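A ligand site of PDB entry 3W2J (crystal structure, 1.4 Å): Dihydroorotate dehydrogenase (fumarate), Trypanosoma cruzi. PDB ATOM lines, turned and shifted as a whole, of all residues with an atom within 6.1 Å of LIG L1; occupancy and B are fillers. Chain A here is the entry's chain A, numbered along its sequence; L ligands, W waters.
A fluorine (F2) of LIG L1 lies close to the side-chain amino group of Lys 215, at 3.4 Å. Ser 69 touches LIG L1. O of Ser 130 touches O4 of LIG L1, 3.6 Å away. Pro 132 touches LIG L1 (CD to C13, 3.6 Å). Hydrophobic or aromatic side chains within 4 Å of LIG L1: Met 70, Leu 72 and Pro 132. Of the 22 residues printed, 12 come within 4 Å of LIG L1.
OD1 of Asn 68 lies within hydrogen-bond range of N of Met 70, at 3.4 Å. The side-chain hydroxyl (OG) of Ser 130 lies within hydrogen-bond range of the backbone carbonyl oxygen (O) of Lys 165. ND2 of Asn 195 is in hydrogen-bond range of OD1 of Asn 128. The side-chain amide oxygen (OD1) of Asn 199 is in hydrogen-bond range of the side-chain amino group (NZ) of Lys 215, 2.8 Å away. The side-chain amide oxygen (OD1) of Asn 195 is in hydrogen-bond range of the side-chain hydroxyl (OG) of Ser 196, at 3.4 Å. N of Gly 71 sits close to ND2 of Asn 54, at 3.5 Å. ND2 of Asn 195 sits at hydrogen-bond distance from OG of Ser 130. The backbone NH (N) of Asn 54 sits at hydrogen-bond distance from the backbone carbonyl oxygen (O) of Met 70 (2.9 Å).
A nitrogen (N2) of LIG L1 sits close to a nitrogen (N1) of LG2 L2, 3.5 Å away.
Water W3 lies within hydrogen-bond range of the side-chain amide nitrogen of Asn 199 (3.1 Å) and the side-chain amino group of Lys 215 (3.2 Å). Water W4 bridges O of Asn 68 (2.9 Å) and O1 of LIG L1 (3.0 Å). Water W5 bridges OG of Ser 69 (2.8 Å) and NZ of Lys 215 (2.9 Å). Water W1 lies within hydrogen-bond range of the backbone NH (N) of Asn 199 (2.9 Å) and the backbone NH (N) of Gly 220 (3.2 Å).
An oxygen (O4) of LIG L1 sits at hydrogen-bond distance from the side-chain amide nitrogen (ND2) of Asn 128. ND2 of Asn 128 lies within hydrogen-bond range of O1 of LG2 L2 (3.4 Å). N of Met 70 sits at hydrogen-bond distance from O1 of LIG L1 (3.1 Å). The side-chain amide nitrogen (ND2) of Asn 195 is in hydrogen-bond range of an oxygen (O1) of LG2 L2 (3.4 Å). The side-chain amide nitrogen (ND2) of Asn 68 is in hydrogen-bond range of an oxygen (O3) of LIG L1, 2.9 Å away. An oxygen (O3) of LIG L1 sits at hydrogen-bond distance from the side-chain hydroxyl of Ser 196 (2.8 Å). O3 of LG2 L2 is in hydrogen-bond range of NZ of Lys 165 (2.8 Å). An oxygen (O1) of LIG L1 lies within hydrogen-bond range of the backbone NH of Gly 71 (3.3 Å). O of Ala 20 is in hydrogen-bond range of O3 of LG2 L2 (2.8 Å). NZ of Lys 44 sits at hydrogen-bond distance from O2 of LG2 L2, at 2.8 Å. N2 of LG2 L2 sits at hydrogen-bond distance from OG of Ser 45 (2.8 Å). NZ of Lys 44 is in salt-bridge range of O2 of LIG L1, at 3.3 Å. A nitrogen (N2) of LIG L1 lies within hydrogen-bond range of the side-chain amide oxygen (OD1) of Asn 195. An oxygen (O2) of LIG L1 sits at hydrogen-bond distance from the backbone NH (N) of Leu 72 (2.9 Å).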
ATOM      1  N   ALA A  20     -34.410  -6.366   8.269  1.00  0.00           N
ATOM      2  CA  ALA A  20     -34.199  -7.544   9.036  1.00  0.00           C
ATOM      3  C   ALA A  20     -34.277  -7.194  10.498  1.00  0.00           C
ATOM      4  O   ALA A  20     -33.791  -6.160  10.999  1.00  0.00           O
ATOM      5  CB  ALA A  20     -32.862  -8.209   8.683  1.00  0.00           C
ATOM      6  N   LYS A  44     -35.706 -12.689  10.158  1.00  0.00           N
ATOM      7  CA  LYS A  44     -34.818 -12.321  11.210  1.00  0.00           C
ATOM      8  C   LYS A  44     -33.432 -12.951  11.038  1.00  0.00           C
ATOM      9  O   LYS A  44     -33.396 -14.170  10.808  1.00  0.00           O
ATOM     10  CB  LYS A  44     -35.412 -12.732  12.564  1.00  0.00           C
ATOM     11  CG  LYS A  44     -34.484 -12.554  13.759  1.00  0.00           C
ATOM     12  CD  LYS A  44     -34.099 -11.071  14.178  1.00  0.00           C
ATOM     13  CE  LYS A  44     -32.895 -10.964  15.127  1.00  0.00           C
ATOM     14  NZ  LYS A  44     -32.513  -9.492  15.565  1.00  0.00           N
ATOM     15  N   SER A  45     -32.407 -12.165  11.215  1.00  0.00           N
ATOM     16  CA  SER A  45     -31.042 -12.722  11.107  1.00  0.00           C
ATOM     17  C   SER A  45     -30.930 -13.876  12.109  1.00  0.00           C
ATOM     18  O   SER A  45     -31.281 -13.767  13.271  1.00  0.00           O
ATOM     19  CB  SER A  45     -29.987 -11.749  11.495  1.00  0.00           C
ATOM     20  OG  SER A  45     -29.935 -10.702  10.536  1.00  0.00           O
ATOM     21  N   ASN A  54     -30.840 -10.852  24.570  1.00  0.00           N
ATOM     22  CA  ASN A  54     -30.486 -10.150  25.784  1.00  0.00           C
ATOM     23  C   ASN A  54     -31.663  -9.899  26.703  1.00  0.00           C
ATOM     24  O   ASN A  54     -32.787  -9.948  26.313  1.00  0.00           O
ATOM     25  CB  ASN A  54     -29.893  -8.782  25.422  1.00  0.00           C
ATOM     26  CG  ASN A  54     -28.518  -8.869  24.904  1.00  0.00           C
ATOM     27  OD1 ASN A  54     -27.783  -9.878  25.184  1.00  0.00           O
ATOM     28  ND2 ASN A  54     -28.059  -7.920  24.091  1.00  0.00           N
ATOM     29  N   ASN A  68     -31.537  -0.126  20.135  1.00  0.00           N
ATOM     30  CA  ASN A  68     -31.705  -1.561  20.446  1.00  0.00           C
ATOM     31  C   ASN A  68     -30.385  -2.233  20.706  1.00  0.00           C
ATOM     32  O   ASN A  68     -29.373  -2.016  20.076  1.00  0.00           O
ATOM     33  CB  ASN A  68     -32.509  -2.349  19.382  1.00  0.00           C
ATOM     34  CG  ASN A  68     -31.628  -2.842  18.272  1.00  0.00           C
ATOM     35  OD1 ASN A  68     -31.007  -3.927  18.385  1.00  0.00           O
ATOM     36  ND2 ASN A  68     -31.538  -2.126  17.182  1.00  0.00           N
ATOM     37  N   SER A  69     -30.415  -3.147  21.641  1.00  0.00           N
ATOM     38  CA  SER A  69     -29.383  -4.179  21.836  1.00  0.00           C
ATOM     39  C   SER A  69     -30.057  -5.518  22.031  1.00  0.00           C
ATOM     40  O   SER A  69     -30.077  -6.042  23.152  1.00  0.00           O
ATOM     41  CB  SER A  69     -28.424  -3.800  22.962  1.00  0.00           C
ATOM     42  OG  SER A  69     -27.637  -2.685  22.593  1.00  0.00           O
ATOM     43  N   MET A  70     -30.698  -6.024  20.993  1.00  0.00           N
ATOM     44  CA  MET A  70     -31.552  -7.196  21.128  1.00  0.00           C
ATOM     45  C   MET A  70     -30.767  -8.437  21.534  1.00  0.00           C
ATOM     46  O   MET A  70     -31.284  -9.316  22.196  1.00  0.00           O
ATOM     47  CB  MET A  70     -32.214  -7.469  19.806  1.00  0.00           C
ATOM     48  CG  MET A  70     -33.119  -6.401  19.243  1.00  0.00           C
ATOM     49  SD  MET A  70     -34.442  -5.861  20.349  1.00  0.00           S
ATOM     50  CE  MET A  70     -35.502  -7.170  20.305  1.00  0.00           C
ATOM     51  N   GLY A  71     -29.537  -8.589  21.040  1.00  0.00           N
ATOM     52  CA  GLY A  71     -28.745  -9.785  21.282  1.00  0.00           C
ATOM     53  C   GLY A  71     -29.018 -10.902  20.323  1.00  0.00           C
ATOM     54  O   GLY A  71     -28.858 -12.073  20.701  1.00  0.00           O
ATOM     55  N   LEU A  72     -29.499 -10.625  19.147  1.00  0.00           N
ATOM     56  CA  LEU A  72     -29.789 -11.596  18.159  1.00  0.00           C
ATOM     57  C   LEU A  72     -30.749 -12.690  18.613  1.00  0.00           C
ATOM     58  O   LEU A  72     -30.526 -13.884  18.316  1.00  0.00           O
ATOM     59  CB  LEU A  72     -28.480 -12.117  17.576  1.00  0.00           C
ATOM     60  CG  LEU A  72     -28.263 -12.722  16.229  1.00  0.00           C
ATOM     61  CD1 LEU A  72     -29.000 -12.006  15.162  1.00  0.00           C
ATOM     62  CD2 LEU A  72     -26.752 -12.695  15.993  1.00  0.00           C
ATOM     63  N   PRO A  73     -31.834 -12.397  19.237  1.00  0.00           N
ATOM     64  CA  PRO A  73     -32.883 -13.412  19.533  1.00  0.00           C
ATOM     65  C   PRO A  73     -33.427 -13.960  18.235  1.00  0.00           C
ATOM     66  O   PRO A  73     -33.719 -13.205  17.305  1.00  0.00           O
ATOM     67  CB  PRO A  73     -33.928 -12.685  20.294  1.00  0.00           C
ATOM     68  CG  PRO A  73     -33.835 -11.255  19.845  1.00  0.00           C
ATOM     69  CD  PRO A  73     -32.371 -11.004  19.437  1.00  0.00           C
ATOM     70  N   SER A 100     -26.751 -14.421  10.340  1.00  0.00           N
ATOM     71  CA  SER A 100     -25.774 -13.653  11.112  1.00  0.00           C
ATOM     72  C   SER A 100     -25.040 -14.570  12.088  1.00  0.00           C
ATOM     73  O   SER A 100     -25.085 -14.413  13.316  1.00  0.00           O
ATOM     74  CB  SER A 100     -26.521 -12.516  11.781  1.00  0.00           C
ATOM     75  OG  SER A 100     -25.624 -11.725  12.536  1.00  0.00           O
ATOM     76  N   LEU A 102     -22.068 -16.290  14.247  1.00  0.00           N
ATOM     77  CA  LEU A 102     -21.121 -15.675  15.168  1.00  0.00           C
ATOM     78  C   LEU A 102     -19.654 -15.958  14.885  1.00  0.00           C
ATOM     79  O   LEU A 102     -18.751 -15.421  15.574  1.00  0.00           O
ATOM     80  CB  LEU A 102     -21.540 -16.008  16.602  1.00  0.00           C
ATOM     81  CG  LEU A 102     -22.926 -15.177  16.952  1.00  0.00           C
ATOM     82  CD1 LEU A 102     -23.459 -15.638  18.274  1.00  0.00           C
ATOM     83  CD2 LEU A 102     -22.783 -13.654  16.932  1.00  0.00           C
ATOM     84  N   ASN A 128     -25.547 -10.812   6.993  1.00  0.00           N
ATOM     85  CA  ASN A 128     -25.326  -9.695   7.886  1.00  0.00           C
ATOM     86  C   ASN A 128     -23.866  -9.609   8.362  1.00  0.00           C
ATOM     87  O   ASN A 128     -23.455 -10.359   9.105  1.00  0.00           O
ATOM     88  CB  ASN A 128     -26.243  -9.848   9.091  1.00  0.00           C
ATOM     89  CG  ASN A 128     -26.202  -8.672  10.026  1.00  0.00           C
ATOM     90  OD1 ASN A 128     -25.631  -7.694   9.788  1.00  0.00           O
ATOM     91  ND2 ASN A 128     -26.929  -8.801  11.076  1.00  0.00           N
ATOM     92  N   SER A 130     -22.656  -6.747   9.776  1.00  0.00           N
ATOM     93  CA  SER A 130     -22.678  -5.680  10.776  1.00  0.00           C
ATOM     94  C   SER A 130     -23.012  -6.412  12.000  1.00  0.00           C
ATOM     95  O   SER A 130     -24.085  -6.330  12.495  1.00  0.00           O
ATOM     96  CB  SER A 130     -23.730  -4.597  10.461  1.00  0.00           C
ATOM     97  OG  SER A 130     -24.428  -4.803   9.102  1.00  0.00           O
ATOM     98  N   CYS A 131     -22.099  -7.244  12.423  1.00  0.00           N
ATOM     99  CA  CYS A 131     -22.289  -8.266  13.351  1.00  0.00           C
ATOM    100  C   CYS A 131     -20.962  -8.505  14.180  1.00  0.00           C
ATOM    101  O   CYS A 131     -19.884  -8.484  13.648  1.00  0.00           O
ATOM    102  CB  CYS A 131     -22.462  -9.583  12.504  1.00  0.00           C
ATOM    103  SG  CYS A 131     -22.976 -11.035  13.483  1.00  0.00           S
ATOM    104  N   PRO A 132     -21.130  -8.923  15.510  1.00  0.00           N
ATOM    105  CA  PRO A 132     -19.899  -9.338  16.211  1.00  0.00           C
ATOM    106  C   PRO A 132     -19.118 -10.552  15.706  1.00  0.00           C
ATOM    107  O   PRO A 132     -19.627 -11.501  15.214  1.00  0.00           O
ATOM    108  CB  PRO A 132     -20.401  -9.697  17.632  1.00  0.00           C
ATOM    109  CG  PRO A 132     -21.662  -8.964  17.840  1.00  0.00           C
ATOM    110  CD  PRO A 132     -22.307  -9.137  16.501  1.00  0.00           C
ATOM    111  N   LYS A 165     -25.586  -7.148   4.164  1.00  0.00           N
ATOM    112  CA  LYS A 165     -26.103  -6.042   5.014  1.00  0.00           C
ATOM    113  C   LYS A 165     -24.908  -5.393   5.653  1.00  0.00           C
ATOM    114  O   LYS A 165     -24.120  -6.028   6.382  1.00  0.00           O
ATOM    115  CB  LYS A 165     -27.035  -6.555   6.052  1.00  0.00           C
ATOM    116  CG  LYS A 165     -27.680  -5.561   6.996  1.00  0.00           C
ATOM    117  CD  LYS A 165     -28.680  -4.622   6.400  1.00  0.00           C
ATOM    118  CE  LYS A 165     -29.478  -3.844   7.408  1.00  0.00           C
ATOM    119  NZ  LYS A 165     -30.405  -4.664   8.205  1.00  0.00           N
ATOM    120  N   ASN A 195     -27.312  -0.937   8.303  1.00  0.00           N
ATOM    121  CA  ASN A 195     -27.600  -1.389   9.641  1.00  0.00           C
ATOM    122  C   ASN A 195     -27.618  -0.176  10.590  1.00  0.00           C
ATOM    123  O   ASN A 195     -27.391   0.895  10.184  1.00  0.00           O
ATOM    124  CB  ASN A 195     -26.634  -2.536  10.101  1.00  0.00           C
ATOM    125  CG  ASN A 195     -27.330  -3.585  10.996  1.00  0.00           C
ATOM    126  OD1 ASN A 195     -27.989  -3.260  11.928  1.00  0.00           O
ATOM    127  ND2 ASN A 195     -27.131  -4.842  10.672  1.00  0.00           N
ATOM    128  N   SER A 196     -27.901  -0.473  11.837  1.00  0.00           N
ATOM    129  CA  SER A 196     -27.971   0.623  12.777  1.00  0.00           C
ATOM    130  C   SER A 196     -26.672   1.385  12.978  1.00  0.00           C
ATOM    131  O   SER A 196     -25.631   0.901  12.778  1.00  0.00           O
ATOM    132  CB  SER A 196     -28.575   0.174  14.109  1.00  0.00           C
ATOM    133  OG  SER A 196     -28.216  -1.013  14.513  1.00  0.00           O
ATOM    134  N   ASN A 199     -23.857   1.726  18.758  1.00  0.00           N
ATOM    135  CA  ASN A 199     -23.413   2.164  20.100  1.00  0.00           C
ATOM    136  C   ASN A 199     -23.736   3.583  20.370  1.00  0.00           C
ATOM    137  O   ASN A 199     -22.836   4.315  20.912  1.00  0.00           O
ATOM    138  CB  ASN A 199     -21.968   1.734  20.328  1.00  0.00           C
ATOM    139  CG  ASN A 199     -21.837   0.270  20.287  1.00  0.00           C
ATOM    140  OD1 ASN A 199     -22.419  -0.396  21.208  1.00  0.00           O
ATOM    141  ND2 ASN A 199     -21.164  -0.301  19.320  1.00  0.00           N
ATOM    142  N   LYS A 215     -25.562  -3.760  27.818  1.00  0.00           N
ATOM    143  CA  LYS A 215     -24.468  -2.958  27.392  1.00  0.00           C
ATOM    144  C   LYS A 215     -24.492  -1.608  28.044  1.00  0.00           C
ATOM    145  O   LYS A 215     -24.083  -0.591  27.482  1.00  0.00           O
ATOM    146  CB  LYS A 215     -24.456  -2.820  25.883  1.00  0.00           C
ATOM    147  CG  LYS A 215     -24.182  -4.150  25.140  1.00  0.00           C
ATOM    148  CD  LYS A 215     -24.295  -3.984  23.595  1.00  0.00           C
ATOM    149  CE  LYS A 215     -23.436  -2.854  23.076  1.00  0.00           C
ATOM    150  NZ  LYS A 215     -23.330  -2.986  21.550  1.00  0.00           N
ATOM    151  N   GLY A 220     -27.720   0.123  19.124  1.00  0.00           N
ATOM    152  CA  GLY A 220     -27.758   0.658  17.738  1.00  0.00           C
ATOM    153  C   GLY A 220     -28.956   1.534  17.505  1.00  0.00           C
ATOM    154  O   GLY A 220     -30.063   1.276  17.989  1.00  0.00           O
HETATM  155  O1  LIG L   1     -28.890  -6.590  18.511  1.00  0.00           O
HETATM  156  C1  LIG L   1     -29.335  -7.311  17.603  1.00  0.00           C
HETATM  157  O2  LIG L   1     -29.995  -8.390  17.396  1.00  0.00           O
HETATM  158  C2  LIG L   1     -29.108  -6.550  16.197  1.00  0.00           C
HETATM  159  N1  LIG L   1     -29.631  -5.230  16.152  1.00  0.00           N
HETATM  160  C3  LIG L   1     -29.407  -4.404  15.127  1.00  0.00           C
HETATM  161  O3  LIG L   1     -29.819  -3.231  15.147  1.00  0.00           O
HETATM  162  N2  LIG L   1     -28.749  -4.897  14.061  1.00  0.00           N
HETATM  163  C4  LIG L   1     -28.229  -6.194  13.959  1.00  0.00           C
HETATM  164  O4  LIG L   1     -27.626  -6.589  12.955  1.00  0.00           O
HETATM  165  C5  LIG L   1     -28.439  -7.019  15.099  1.00  0.00           C
HETATM  166  C6  LIG L   1     -27.900  -8.370  15.131  1.00  0.00           C
HETATM  167  C7  LIG L   1     -26.322  -8.323  15.310  1.00  0.00           C
HETATM  168  C8  LIG L   1     -25.795  -7.754  16.468  1.00  0.00           C
HETATM  169  C9  LIG L   1     -25.422  -6.374  16.534  1.00  0.00           C
HETATM  170  C10 LIG L   1     -24.932  -5.776  17.728  1.00  0.00           C
HETATM  171  F1  LIG L   1     -24.632  -4.446  17.791  1.00  0.00           F
HETATM  172  C11 LIG L   1     -24.830  -6.526  18.868  1.00  0.00           C
HETATM  173  F2  LIG L   1     -24.346  -5.865  20.016  1.00  0.00           F
HETATM  174  C12 LIG L   1     -25.181  -7.858  18.876  1.00  0.00           C
HETATM  175  C13 LIG L   1     -25.654  -8.537  17.710  1.00  0.00           C
HETATM  176  N1  LG2 L   2     -30.434  -5.751  11.153  1.00  0.00           N
HETATM  177  C1  LG2 L   2     -30.073  -6.999  10.708  1.00  0.00           C
HETATM  178  O1  LG2 L   2     -29.462  -7.064   9.634  1.00  0.00           O
HETATM  179  N2  LG2 L   2     -30.402  -8.125  11.385  1.00  0.00           N
HETATM  180  C2  LG2 L   2     -31.125  -8.093  12.525  1.00  0.00           C
HETATM  181  O2  LG2 L   2     -31.461  -9.198  13.033  1.00  0.00           O
HETATM  182  C3  LG2 L   2     -31.569  -6.887  13.041  1.00  0.00           C
HETATM  183  N3  LG2 L   2     -32.318  -6.773  14.169  1.00  0.00           N
HETATM  184  C4  LG2 L   2     -32.912  -5.611  14.453  1.00  0.00           C
HETATM  185  C5  LG2 L   2     -33.807  -5.547  15.535  1.00  0.00           C
HETATM  186  C6  LG2 L   2     -34.482  -4.389  15.819  1.00  0.00           C
HETATM  187  C7  LG2 L   2     -35.526  -4.361  16.959  1.00  0.00           C
HETATM  188  C8  LG2 L   2     -34.193  -3.206  15.125  1.00  0.00           C
HETATM  189  C9  LG2 L   2     -34.856  -1.875  15.415  1.00  0.00           C
HETATM  190  C10 LG2 L   2     -33.275  -3.239  14.114  1.00  0.00           C
HETATM  191  C11 LG2 L   2     -32.629  -4.413  13.741  1.00  0.00           C
HETATM  192  N4  LG2 L   2     -31.678  -4.502  12.675  1.00  0.00           N
HETATM  193  C12 LG2 L   2     -31.249  -5.735  12.254  1.00  0.00           C
HETATM  194  C13 LG2 L   2     -31.344  -3.268  11.933  1.00  0.00           C
HETATM  195  C14 LG2 L   2     -32.430  -2.882  10.931  1.00  0.00           C
HETATM  196  O3  LG2 L   2     -32.513  -3.931   9.928  1.00  0.00           O
HETATM  197  C15 LG2 L   2     -32.104  -1.624  10.216  1.00  0.00           C
HETATM  198  O4  LG2 L   2     -30.866  -1.807   9.528  1.00  0.00           O
HETATM  199  C16 LG2 L   2     -31.889  -0.404  11.188  1.00  0.00           C
HETATM  200  O5  LG2 L   2     -32.951  -0.468  12.180  1.00  0.00           O
HETATM  201  C17 LG2 L   2     -32.059   0.912  10.435  1.00  0.00           C
HETATM  202  O6  LG2 L   2     -33.271   1.098   9.761  1.00  0.00           O
HETATM  203  P1  LG2 L   2     -34.434   2.042  10.371  1.00  0.00           P
HETATM  204  O7  LG2 L   2     -35.602   1.880   9.389  1.00  0.00           O
HETATM  205  O8  LG2 L   2     -33.886   3.421  10.487  1.00  0.00           O
HETATM  206  O9  LG2 L   2     -34.769   1.463  11.778  1.00  0.00           O
HETATM  207  O   HOH W   1     -24.768  -1.062  18.491  1.00  0.00           O
HETATM  208  O   HOH W   2     -27.315  -6.483  21.110  1.00  0.00           O
HETATM  209  O   HOH W   3     -22.504  -2.967  18.472  1.00  0.00           O
HETATM  210  O   HOH W   4     -27.724  -3.805  18.417  1.00  0.00           O
HETATM  211  O   HOH W   5     -25.969  -2.974  20.303  1.00  0.00           O
